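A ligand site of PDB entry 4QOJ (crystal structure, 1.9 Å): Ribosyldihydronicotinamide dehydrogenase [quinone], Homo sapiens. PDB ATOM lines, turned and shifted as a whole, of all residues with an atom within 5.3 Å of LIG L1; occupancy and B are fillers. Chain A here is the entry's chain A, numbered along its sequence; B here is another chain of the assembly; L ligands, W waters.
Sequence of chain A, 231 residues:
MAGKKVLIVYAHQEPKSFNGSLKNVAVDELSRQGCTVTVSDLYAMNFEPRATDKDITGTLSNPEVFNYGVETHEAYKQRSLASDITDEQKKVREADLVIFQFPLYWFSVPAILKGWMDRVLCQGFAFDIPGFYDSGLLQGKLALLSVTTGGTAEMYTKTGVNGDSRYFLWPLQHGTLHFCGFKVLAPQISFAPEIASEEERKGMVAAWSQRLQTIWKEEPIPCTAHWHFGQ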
ATOM      1  N   HIS A  12     -11.970  -2.310 -29.739  1.00  0.00           N
ATOM      2  CA  HIS A  12     -10.889  -1.370 -29.464  1.00  0.00           C
ATOM      3  C   HIS A  12     -10.645  -0.547 -30.717  1.00  0.00           C
ATOM      4  O   HIS A  12     -10.666  -1.079 -31.827  1.00  0.00           O
ATOM      5  CB  HIS A  12      -9.603  -2.039 -28.950  1.00  0.00           C
ATOM      6  CG  HIS A  12      -8.770  -1.102 -28.120  1.00  0.00           C
ATOM      7  ND1 HIS A  12      -8.047  -0.074 -28.706  1.00  0.00           N
ATOM      8  CD2 HIS A  12      -8.601  -1.039 -26.780  1.00  0.00           C
ATOM      9  CE1 HIS A  12      -7.464   0.566 -27.707  1.00  0.00           C
ATOM     10  NE2 HIS A  12      -7.743   0.000 -26.538  1.00  0.00           N
ATOM     11  N   SER A  17      -2.891  -1.229 -29.882  1.00  0.00           N
ATOM     12  CA  SER A  17      -3.114  -1.330 -28.442  1.00  0.00           C
ATOM     13  C   SER A  17      -2.815  -2.730 -27.906  1.00  0.00           C
ATOM     14  O   SER A  17      -2.662  -3.678 -28.690  1.00  0.00           O
ATOM     15  CB  SER A  17      -4.538  -0.930 -28.079  1.00  0.00           C
ATOM     16  OG  SER A  17      -5.471  -1.879 -28.577  1.00  0.00           O
ATOM     17  N   PHE A  18      -2.800  -2.849 -26.571  1.00  0.00           N
ATOM     18  CA  PHE A  18      -2.643  -4.112 -25.863  1.00  0.00           C
ATOM     19  C   PHE A  18      -3.833  -4.995 -26.221  1.00  0.00           C
ATOM     20  O   PHE A  18      -3.640  -6.185 -26.467  1.00  0.00           O
ATOM     21  CB  PHE A  18      -2.552  -3.878 -24.358  1.00  0.00           C
ATOM     22  CG  PHE A  18      -2.217  -5.122 -23.572  1.00  0.00           C
ATOM     23  CD1 PHE A  18      -0.918  -5.614 -23.517  1.00  0.00           C
ATOM     24  CD2 PHE A  18      -3.207  -5.819 -22.893  1.00  0.00           C
ATOM     25  CE1 PHE A  18      -0.615  -6.763 -22.789  1.00  0.00           C
ATOM     26  CE2 PHE A  18      -2.904  -6.969 -22.165  1.00  0.00           C
ATOM     27  CZ  PHE A  18      -1.622  -7.440 -22.119  1.00  0.00           C
ATOM     28  N   ASN A  19      -5.066  -4.417 -26.322  1.00  0.00           N
ATOM     29  CA  ASN A  19      -6.240  -5.190 -26.754  1.00  0.00           C
ATOM     30  C   ASN A  19      -6.009  -5.735 -28.166  1.00  0.00           C
ATOM     31  O   ASN A  19      -6.368  -6.879 -28.436  1.00  0.00           O
ATOM     32  CB  ASN A  19      -7.520  -4.327 -26.733  1.00  0.00           C
ATOM     33  CG  ASN A  19      -8.205  -4.417 -25.401  1.00  0.00           C
ATOM     34  OD1 ASN A  19      -9.046  -5.292 -25.179  1.00  0.00           O
ATOM     35  ND2 ASN A  19      -7.790  -3.573 -24.458  1.00  0.00           N
ATOM     36  N   GLY A  20      -5.446  -4.909 -29.044  1.00  0.00           N
ATOM     37  CA  GLY A  20      -5.103  -5.294 -30.418  1.00  0.00           C
ATOM     38  C   GLY A  20      -4.138  -6.475 -30.442  1.00  0.00           C
ATOM     39  O   GLY A  20      -4.347  -7.427 -31.200  1.00  0.00           O
ATOM     40  N   PRO A 103     -11.473  -3.554 -23.640  1.00  0.00           N
ATOM     41  CA  PRO A 103     -11.041  -2.884 -22.410  1.00  0.00           C
ATOM     42  C   PRO A 103     -12.295  -2.673 -21.545  1.00  0.00           C
ATOM     43  O   PRO A 103     -13.394  -2.392 -22.057  1.00  0.00           O
ATOM     44  CB  PRO A 103     -10.509  -1.541 -22.907  1.00  0.00           C
ATOM     45  CG  PRO A 103     -11.298  -1.248 -24.166  1.00  0.00           C
ATOM     46  CD  PRO A 103     -11.691  -2.581 -24.742  1.00  0.00           C
ATOM     47  N   LEU A 104     -12.111  -2.768 -20.240  1.00  0.00           N
ATOM     48  CA  LEU A 104     -13.174  -2.522 -19.286  1.00  0.00           C
ATOM     49  C   LEU A 104     -13.535  -1.042 -19.307  1.00  0.00           C
ATOM     50  O   LEU A 104     -12.659  -0.187 -19.120  1.00  0.00           O
ATOM     51  CB  LEU A 104     -12.735  -2.958 -17.890  1.00  0.00           C
ATOM     52  CG  LEU A 104     -13.855  -3.022 -16.819  1.00  0.00           C
ATOM     53  CD1 LEU A 104     -14.794  -4.197 -17.104  1.00  0.00           C
ATOM     54  CD2 LEU A 104     -13.247  -3.230 -15.411  1.00  0.00           C
ATOM     55  N   TYR A 105     -14.818  -0.745 -19.556  1.00  0.00           N
ATOM     56  CA  TYR A 105     -15.318   0.627 -19.530  1.00  0.00           C
ATOM     57  C   TYR A 105     -16.432   0.664 -18.486  1.00  0.00           C
ATOM     58  O   TYR A 105     -17.465   0.015 -18.654  1.00  0.00           O
ATOM     59  CB  TYR A 105     -15.941   1.044 -20.899  1.00  0.00           C
ATOM     60  CG  TYR A 105     -15.025   1.602 -21.965  1.00  0.00           C
ATOM     61  CD1 TYR A 105     -13.647   1.346 -21.947  1.00  0.00           C
ATOM     62  CD2 TYR A 105     -15.539   2.340 -23.029  1.00  0.00           C
ATOM     63  CE1 TYR A 105     -12.816   1.809 -22.973  1.00  0.00           C
ATOM     64  CE2 TYR A 105     -14.719   2.799 -24.063  1.00  0.00           C
ATOM     65  CZ  TYR A 105     -13.357   2.515 -24.036  1.00  0.00           C
ATOM     66  OH  TYR A 105     -12.575   3.013 -25.042  1.00  0.00           O
ATOM     67  N   TRP A 106     -16.224   1.409 -17.409  1.00  0.00           N
ATOM     68  CA  TRP A 106     -17.224   1.562 -16.364  1.00  0.00           C
ATOM     69  C   TRP A 106     -17.725   0.203 -15.829  1.00  0.00           C
ATOM     70  O   TRP A 106     -18.946  -0.038 -15.766  1.00  0.00           O
ATOM     71  CB  TRP A 106     -18.365   2.484 -16.823  1.00  0.00           C
ATOM     72  CG  TRP A 106     -17.916   3.910 -17.055  1.00  0.00           C
ATOM     73  CD1 TRP A 106     -18.115   4.660 -18.168  1.00  0.00           C
ATOM     74  CD2 TRP A 106     -17.196   4.753 -16.128  1.00  0.00           C
ATOM     75  NE1 TRP A 106     -17.511   5.887 -18.030  1.00  0.00           N
ATOM     76  CE2 TRP A 106     -17.001   6.006 -16.760  1.00  0.00           C
ATOM     77  CE3 TRP A 106     -16.759   4.600 -14.800  1.00  0.00           C
ATOM     78  CZ2 TRP A 106     -16.344   7.074 -16.142  1.00  0.00           C
ATOM     79  CZ3 TRP A 106     -16.133   5.678 -14.166  1.00  0.00           C
ATOM     80  CH2 TRP A 106     -15.872   6.868 -14.846  1.00  0.00           C
ATOM     81  N   PHE A 107     -16.768  -0.698 -15.523  1.00  0.00           N
ATOM     82  CA  PHE A 107     -16.985  -2.035 -14.953  1.00  0.00           C
ATOM     83  C   PHE A 107     -17.843  -2.883 -15.892  1.00  0.00           C
ATOM     84  O   PHE A 107     -18.567  -3.776 -15.443  1.00  0.00           O
ATOM     85  CB  PHE A 107     -17.686  -1.912 -13.569  1.00  0.00           C
ATOM     86  CG  PHE A 107     -16.796  -1.719 -12.355  1.00  0.00           C
ATOM     87  CD1 PHE A 107     -15.612  -0.992 -12.439  1.00  0.00           C
ATOM     88  CD2 PHE A 107     -17.209  -2.175 -11.095  1.00  0.00           C
ATOM     89  CE1 PHE A 107     -14.795  -0.838 -11.309  1.00  0.00           C
ATOM     90  CE2 PHE A 107     -16.403  -1.990  -9.961  1.00  0.00           C
ATOM     91  CZ  PHE A 107     -15.215  -1.289 -10.067  1.00  0.00           C
ATOM     92  N   SER A 108     -17.799  -2.555 -17.196  1.00  0.00           N
ATOM     93  CA  SER A 108     -18.616  -3.236 -18.189  1.00  0.00           C
ATOM     94  C   SER A 108     -17.945  -3.190 -19.575  1.00  0.00           C
ATOM     95  O   SER A 108     -16.758  -2.885 -19.694  1.00  0.00           O
ATOM     96  CB  SER A 108     -20.003  -2.591 -18.215  1.00  0.00           C
ATOM     97  OG  SER A 108     -20.896  -3.235 -19.108  1.00  0.00           O
ATOM     98  N   THR A 148      -9.318  -6.204 -20.337  1.00  0.00           N
ATOM     99  CA  THR A 148      -8.149  -5.452 -19.876  1.00  0.00           C
ATOM    100  C   THR A 148      -8.682  -4.347 -18.949  1.00  0.00           C
ATOM    101  O   THR A 148      -9.774  -3.829 -19.174  1.00  0.00           O
ATOM    102  CB  THR A 148      -7.311  -4.898 -21.046  1.00  0.00           C
ATOM    103  OG1 THR A 148      -8.053  -3.858 -21.703  1.00  0.00           O
ATOM    104  CG2 THR A 148      -6.905  -5.988 -22.049  1.00  0.00           C
ATOM    105  N   THR A 149      -7.920  -3.981 -17.921  1.00  0.00           N
ATOM    106  CA  THR A 149      -8.390  -2.940 -16.996  1.00  0.00           C
ATOM    107  C   THR A 149      -7.386  -1.787 -16.870  1.00  0.00           C
ATOM    108  O   THR A 149      -6.216  -1.925 -17.235  1.00  0.00           O
ATOM    109  CB  THR A 149      -8.611  -3.560 -15.586  1.00  0.00           C
ATOM    110  OG1 THR A 149      -7.354  -3.979 -15.072  1.00  0.00           O
ATOM    111  CG2 THR A 149      -9.585  -4.757 -15.581  1.00  0.00           C
ATOM    112  N   GLY A 150      -7.858  -0.661 -16.313  1.00  0.00           N
ATOM    113  CA  GLY A 150      -6.987   0.431 -15.901  1.00  0.00           C
ATOM    114  C   GLY A 150      -6.481   0.122 -14.505  1.00  0.00           C
ATOM    115  O   GLY A 150      -5.292   0.302 -14.212  1.00  0.00           O
ATOM    116  N   GLY A 151      -7.377  -0.396 -13.661  1.00  0.00           N
ATOM    117  CA  GLY A 151      -7.101  -0.754 -12.263  1.00  0.00           C
ATOM    118  C   GLY A 151      -6.200  -1.958 -12.098  1.00  0.00           C
ATOM    119  O   GLY A 151      -6.222  -2.900 -12.909  1.00  0.00           O
ATOM    120  N   TYR A 156      -8.588  -4.659  -7.570  1.00  0.00           N
ATOM    121  CA  TYR A 156      -9.674  -5.580  -7.792  1.00  0.00           C
ATOM    122  C   TYR A 156      -9.691  -6.753  -6.802  1.00  0.00           C
ATOM    123  O   TYR A 156      -9.786  -7.866  -7.184  1.00  0.00           O
ATOM    124  CB  TYR A 156      -9.761  -6.054  -9.251  1.00  0.00           C
ATOM    125  CG  TYR A 156     -10.278  -4.985 -10.175  1.00  0.00           C
ATOM    126  CD1 TYR A 156     -11.619  -4.724 -10.252  1.00  0.00           C
ATOM    127  CD2 TYR A 156      -9.412  -4.248 -10.947  1.00  0.00           C
ATOM    128  CE1 TYR A 156     -12.108  -3.735 -11.077  1.00  0.00           C
ATOM    129  CE2 TYR A 156      -9.887  -3.242 -11.762  1.00  0.00           C
ATOM    130  CZ  TYR A 156     -11.259  -3.005 -11.834  1.00  0.00           C
ATOM    131  OH  TYR A 156     -11.720  -2.017 -12.648  1.00  0.00           O
ATOM    132  N   ASN A 162     -11.884  -1.258  -5.804  1.00  0.00           N
ATOM    133  CA  ASN A 162     -12.803  -1.678  -6.874  1.00  0.00           C
ATOM    134  C   ASN A 162     -13.620  -2.930  -6.580  1.00  0.00           C
ATOM    135  O   ASN A 162     -14.547  -3.256  -7.346  1.00  0.00           O
ATOM    136  CB  ASN A 162     -12.029  -1.864  -8.185  1.00  0.00           C
ATOM    137  CG  ASN A 162     -11.449  -0.596  -8.748  1.00  0.00           C
ATOM    138  OD1 ASN A 162     -11.807   0.512  -8.347  1.00  0.00           O
ATOM    139  ND2 ASN A 162     -10.531  -0.751  -9.681  1.00  0.00           N
ATOM    140  N   PRO A 193      -2.431  -3.070 -18.081  1.00  0.00           N
ATOM    141  CA  PRO A 193      -1.307  -3.162 -19.023  1.00  0.00           C
ATOM    142  C   PRO A 193      -0.596  -1.838 -19.307  1.00  0.00           C
ATOM    143  O   PRO A 193       0.603  -1.863 -19.581  1.00  0.00           O
ATOM    144  CB  PRO A 193      -1.960  -3.708 -20.302  1.00  0.00           C
ATOM    145  CG  PRO A 193      -3.409  -3.345 -20.177  1.00  0.00           C
ATOM    146  CD  PRO A 193      -3.698  -3.508 -18.728  1.00  0.00           C
ATOM    147  N   GLU A 194      -1.337  -0.693 -19.264  1.00  0.00           N
ATOM    148  CA  GLU A 194      -0.769   0.632 -19.555  1.00  0.00           C
ATOM    149  C   GLU A 194       0.343   1.056 -18.610  1.00  0.00           C
ATOM    150  O   GLU A 194       1.274   1.718 -19.049  1.00  0.00           O
ATOM    151  CB  GLU A 194      -1.865   1.707 -19.589  1.00  0.00           C
ATOM    152  CG  GLU A 194      -2.783   1.588 -20.779  1.00  0.00           C
ATOM    153  CD  GLU A 194      -3.982   2.508 -20.694  1.00  0.00           C
ATOM    154  OE1 GLU A 194      -4.833   2.291 -19.785  1.00  0.00           O
ATOM    155  OE2 GLU A 194      -4.061   3.470 -21.485  1.00  0.00           O
ATOM    156  N   TYR B  68      -8.013   6.498 -26.243  1.00  0.00           N
ATOM    157  CA  TYR B  68      -9.249   7.247 -25.960  1.00  0.00           C
ATOM    158  C   TYR B  68      -9.201   8.037 -24.644  1.00  0.00           C
ATOM    159  O   TYR B  68      -9.524   9.224 -24.650  1.00  0.00           O
ATOM    160  CB  TYR B  68     -10.503   6.359 -26.045  1.00  0.00           C
ATOM    161  CG  TYR B  68     -11.777   7.181 -25.949  1.00  0.00           C
ATOM    162  CD1 TYR B  68     -12.290   7.841 -27.060  1.00  0.00           C
ATOM    163  CD2 TYR B  68     -12.433   7.340 -24.730  1.00  0.00           C
ATOM    164  CE1 TYR B  68     -13.438   8.631 -26.971  1.00  0.00           C
ATOM    165  CE2 TYR B  68     -13.590   8.129 -24.626  1.00  0.00           C
ATOM    166  CZ  TYR B  68     -14.098   8.747 -25.753  1.00  0.00           C
ATOM    167  OH  TYR B  68     -15.210   9.542 -25.654  1.00  0.00           O
ATOM    168  N   GLY B  69      -8.828   7.388 -23.549  1.00  0.00           N
ATOM    169  CA  GLY B  69      -8.727   8.026 -22.235  1.00  0.00           C
ATOM    170  C   GLY B  69      -7.791   9.211 -22.216  1.00  0.00           C
ATOM    171  O   GLY B  69      -8.181  10.287 -21.778  1.00  0.00           O
ATOM    172  N   ASP B 118     -19.743   6.444 -20.985  1.00  0.00           N
ATOM    173  CA  ASP B 118     -18.388   6.303 -21.542  1.00  0.00           C
ATOM    174  C   ASP B 118     -17.778   7.617 -22.013  1.00  0.00           C
ATOM    175  O   ASP B 118     -16.605   7.875 -21.756  1.00  0.00           O
ATOM    176  CB  ASP B 118     -18.381   5.324 -22.728  1.00  0.00           C
ATOM    177  CG  ASP B 118     -18.724   3.889 -22.363  1.00  0.00           C
ATOM    178  OD1 ASP B 118     -18.780   3.574 -21.140  1.00  0.00           O
ATOM    179  OD2 ASP B 118     -18.949   3.084 -23.293  1.00  0.00           O
ATOM    180  N   GLY B 175     -18.825   1.218  -9.697  1.00  0.00           N
ATOM    181  CA  GLY B 175     -17.825   1.415 -10.721  1.00  0.00           C
ATOM    182  C   GLY B 175     -17.931   2.712 -11.495  1.00  0.00           C
ATOM    183  O   GLY B 175     -16.985   3.223 -11.934  1.00  0.00           O
HETATM  184  N1  LIG L   1     -10.469   0.696 -16.073  1.00  0.00           N
HETATM  185  C1  LIG L   1     -10.934   0.008 -14.978  1.00  0.00           C
HETATM  186  O1  LIG L   1     -10.172  -0.650 -14.264  1.00  0.00           O
HETATM  187  N2  LIG L   1     -12.278   0.066 -14.655  1.00  0.00           N
HETATM  188  C2  LIG L   1     -13.254   0.795 -15.324  1.00  0.00           C
HETATM  189  O2  LIG L   1     -14.425   0.739 -14.952  1.00  0.00           O
HETATM  190  C3  LIG L   1     -12.745   1.569 -16.445  1.00  0.00           C
HETATM  191  N3  LIG L   1     -13.592   2.353 -17.083  1.00  0.00           N
HETATM  192  C4  LIG L   1     -13.111   3.053 -18.181  1.00  0.00           C
HETATM  193  C5  LIG L   1     -14.004   3.841 -18.922  1.00  0.00           C
HETATM  194  C6  LIG L   1     -13.618   4.463 -20.107  1.00  0.00           C
HETATM  195  C7  LIG L   1     -14.633   5.230 -20.906  1.00  0.00           C
HETATM  196  C8  LIG L   1     -12.282   4.342 -20.537  1.00  0.00           C
HETATM  197  C9  LIG L   1     -11.783   5.074 -21.757  1.00  0.00           C
HETATM  198  C10 LIG L   1     -11.386   3.584 -19.798  1.00  0.00           C
HETATM  199  C11 LIG L   1     -11.775   2.949 -18.616  1.00  0.00           C
HETATM  200  N4  LIG L   1     -10.893   2.130 -17.857  1.00  0.00           N
HETATM  201  C12 LIG L   1     -11.345   1.440 -16.768  1.00  0.00           C
HETATM  202  C13 LIG L   1      -9.499   1.963 -18.304  1.00  0.00           C
HETATM  203  C14 LIG L   1      -9.380   0.922 -19.420  1.00  0.00           C
HETATM  204  O3  LIG L   1      -9.968  -0.318 -19.002  1.00  0.00           O
HETATM  205  C15 LIG L   1      -7.905   0.750 -19.789  1.00  0.00           C
HETATM  206  O4  LIG L   1      -7.453   1.992 -20.317  1.00  0.00           O
HETATM  207  C16 LIG L   1      -7.648  -0.365 -20.806  1.00  0.00           C
HETATM  208  O5  LIG L   1      -8.106  -1.595 -20.259  1.00  0.00           O
HETATM  209  C17 LIG L   1      -6.199  -0.501 -21.242  1.00  0.00           C
HETATM  210  O6  LIG L   1      -6.151  -1.421 -22.369  1.00  0.00           O
HETATM  211  P1  LIG L   1      -5.582  -0.911 -23.813  1.00  0.00           P
HETATM  212  O7  LIG L   1      -5.582  -1.914 -24.856  1.00  0.00           O
HETATM  213  O8  LIG L   1      -6.423   0.312 -24.145  1.00  0.00           O
HETATM  214  O9  LIG L   1      -4.156  -0.371 -23.562  1.00  0.00           O
HETATM  215  C1  LG2 L   2     -10.922   2.218 -12.210  1.00  0.00           C
HETATM  216  C2  LG2 L   2     -12.086   1.945 -11.515  1.00  0.00           C
HETATM  217  C3  LG2 L   2     -13.293   2.460 -11.975  1.00  0.00           C
HETATM  218  C4  LG2 L   2     -13.337   3.235 -13.111  1.00  0.00           C
HETATM  219  C5  LG2 L   2     -12.170   3.532 -13.822  1.00  0.00           C
HETATM  220  C6  LG2 L   2     -10.954   3.008 -13.358  1.00  0.00           C
HETATM  221  C7  LG2 L   2     -12.299   4.450 -14.957  1.00  0.00           C
HETATM  222  C8  LG2 L   2     -11.389   4.900 -15.806  1.00  0.00           C
HETATM  223  C9  LG2 L   2     -11.628   5.835 -16.911  1.00  0.00           C
HETATM  224  C10 LG2 L   2     -10.558   6.200 -17.730  1.00  0.00           C
HETATM  225  C11 LG2 L   2     -10.734   7.042 -18.812  1.00  0.00           C
HETATM  226  C12 LG2 L   2     -11.991   7.562 -19.091  1.00  0.00           C
HETATM  227  C13 LG2 L   2     -13.062   7.247 -18.267  1.00  0.00           C
HETATM  228  C14 LG2 L   2     -12.882   6.380 -17.206  1.00  0.00           C
HETATM  229  O1  LG2 L   2     -12.170   8.317 -20.211  1.00  0.00           O
HETATM  230  O2  LG2 L   2     -14.472   2.300 -11.304  1.00  0.00           O
HETATM  231  O3  LG2 L   2      -9.735   1.711 -11.763  1.00  0.00           O
HETATM  232  O   HOH W   1      -1.908  -0.409 -24.925  1.00  0.00           O
HETATM  233  O   HOH W   2      -8.900   1.897 -23.730  1.00  0.00           O
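Water W1 lies within hydrogen-bond range of O9 of LIG L1 (2.6 Å) and N of Phe 18 (3.1 Å).
OH of Tyr 156 lies close to ND2 of Asn 162 (3.4 Å). O of Thr 148 sits at hydrogen-bond distance from N of Leu 104 (2.8 Å). ND2 of Asn 19 is in hydrogen-bond range of OG1 of Thr 148 (2.8 Å). The side-chain hydroxyl (OG) of Ser 17 sits at hydrogen-bond distance from a ring nitrogen (ND1) of His 12 (3.1 Å). The backbone NH of Asn 19 lies close to the side-chain hydroxyl of Ser 17. The backbone carbonyl oxygen of Gly 151 lies within hydrogen-bond range of the side-chain hydroxyl of Thr 149, at 2.7 Å. The side-chain hydroxyl (OG) of Ser 17 sits at hydrogen-bond distance from the backbone NH (N) of Gly 20, 3.1 Å away.
OH of Tyr 156 is in hydrogen-bond range of O1 of LIG L1, 2.6 Å away. O5 of LIG L1 lies within hydrogen-bond range of O of Thr 148, 3.0 Å away. O5 of LIG L1 lies within hydrogen-bond range of OG1 of Thr 148 (2.7 Å). An oxygen (O4) of LIG L1 lies within hydrogen-bond range of the side-chain carboxylate (OE1) of Glu 194, at 2.7 Å. The backbone NH (N) of Leu 104 lies within hydrogen-bond range of an oxygen (O3) of LIG L1 (3.5 Å). O of Leu 104 sits at hydrogen-bond distance from O3 of LIG L1 (2.7 Å). A ring nitrogen (NE2) of His 12 sits at hydrogen-bond distance from an oxygen (O8) of LIG L1. The backbone NH (N) of Asn 19 sits at hydrogen-bond distance from an oxygen (O7) of LIG L1. The side-chain amide nitrogen of Asn 19 lies within hydrogen-bond range of an oxygen (O7) of LIG L1. The backbone NH (N) of Phe 107 sits at hydrogen-bond distance from an oxygen (O2) of LIG L1, 2.8 Å away. N3 of LIG L1 sits at hydrogen-bond distance from N of Trp 106 (2.8 Å). O1 of LIG L1 sits at hydrogen-bond distance from N of Gly 151. N1 of LIG L1 lies within hydrogen-bond range of N of Gly 150, 3.0 Å away. An oxygen (O5) of LIG L1 lies within hydrogen-bond range of the backbone NH of Thr 149. O7 of LIG L1 lies within hydrogen-bond range of N of Phe 18, at 3.4 Å. O3 of LG2 L2 is in hydrogen-bond range of ND2 of Asn 162 (3.3 Å). The backbone carbonyl oxygen (O) of Gly 175 of chain B sits at hydrogen-bond distance from an oxygen (O2) of LG2 L2, at 2.8 Å.
Residues that only touch LIG L1: Asp 118 of chain B, Tyr 105, Ser 17, Pro 103 and Tyr 68 of chain B. Hydrophobic or aromatic side chains within 4 Å of LIG L1: His 12, Phe 18, Pro 103, Leu 104, Tyr 105, Phe 107, Tyr 156 and Tyr 68 of chain B. 17 residues have an atom within 4 Å of LIG L1: His 12, Ser 17, Phe 18, Asn 19, Pro 103, Leu 104, Tyr 105, Trp 106, Phe 107, Thr 148, Thr 149, Gly 150, Gly 151, Tyr 156, Glu 194, Tyr 68 of chain B and Asp 118 of chain B. The nearest printed residue that does not touch LIG L1 is Pro 193 (4.003 Å).
An oxygen (O3) of LG2 L2 is in hydrogen-bond range of an oxygen (O1) of LIG L1.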
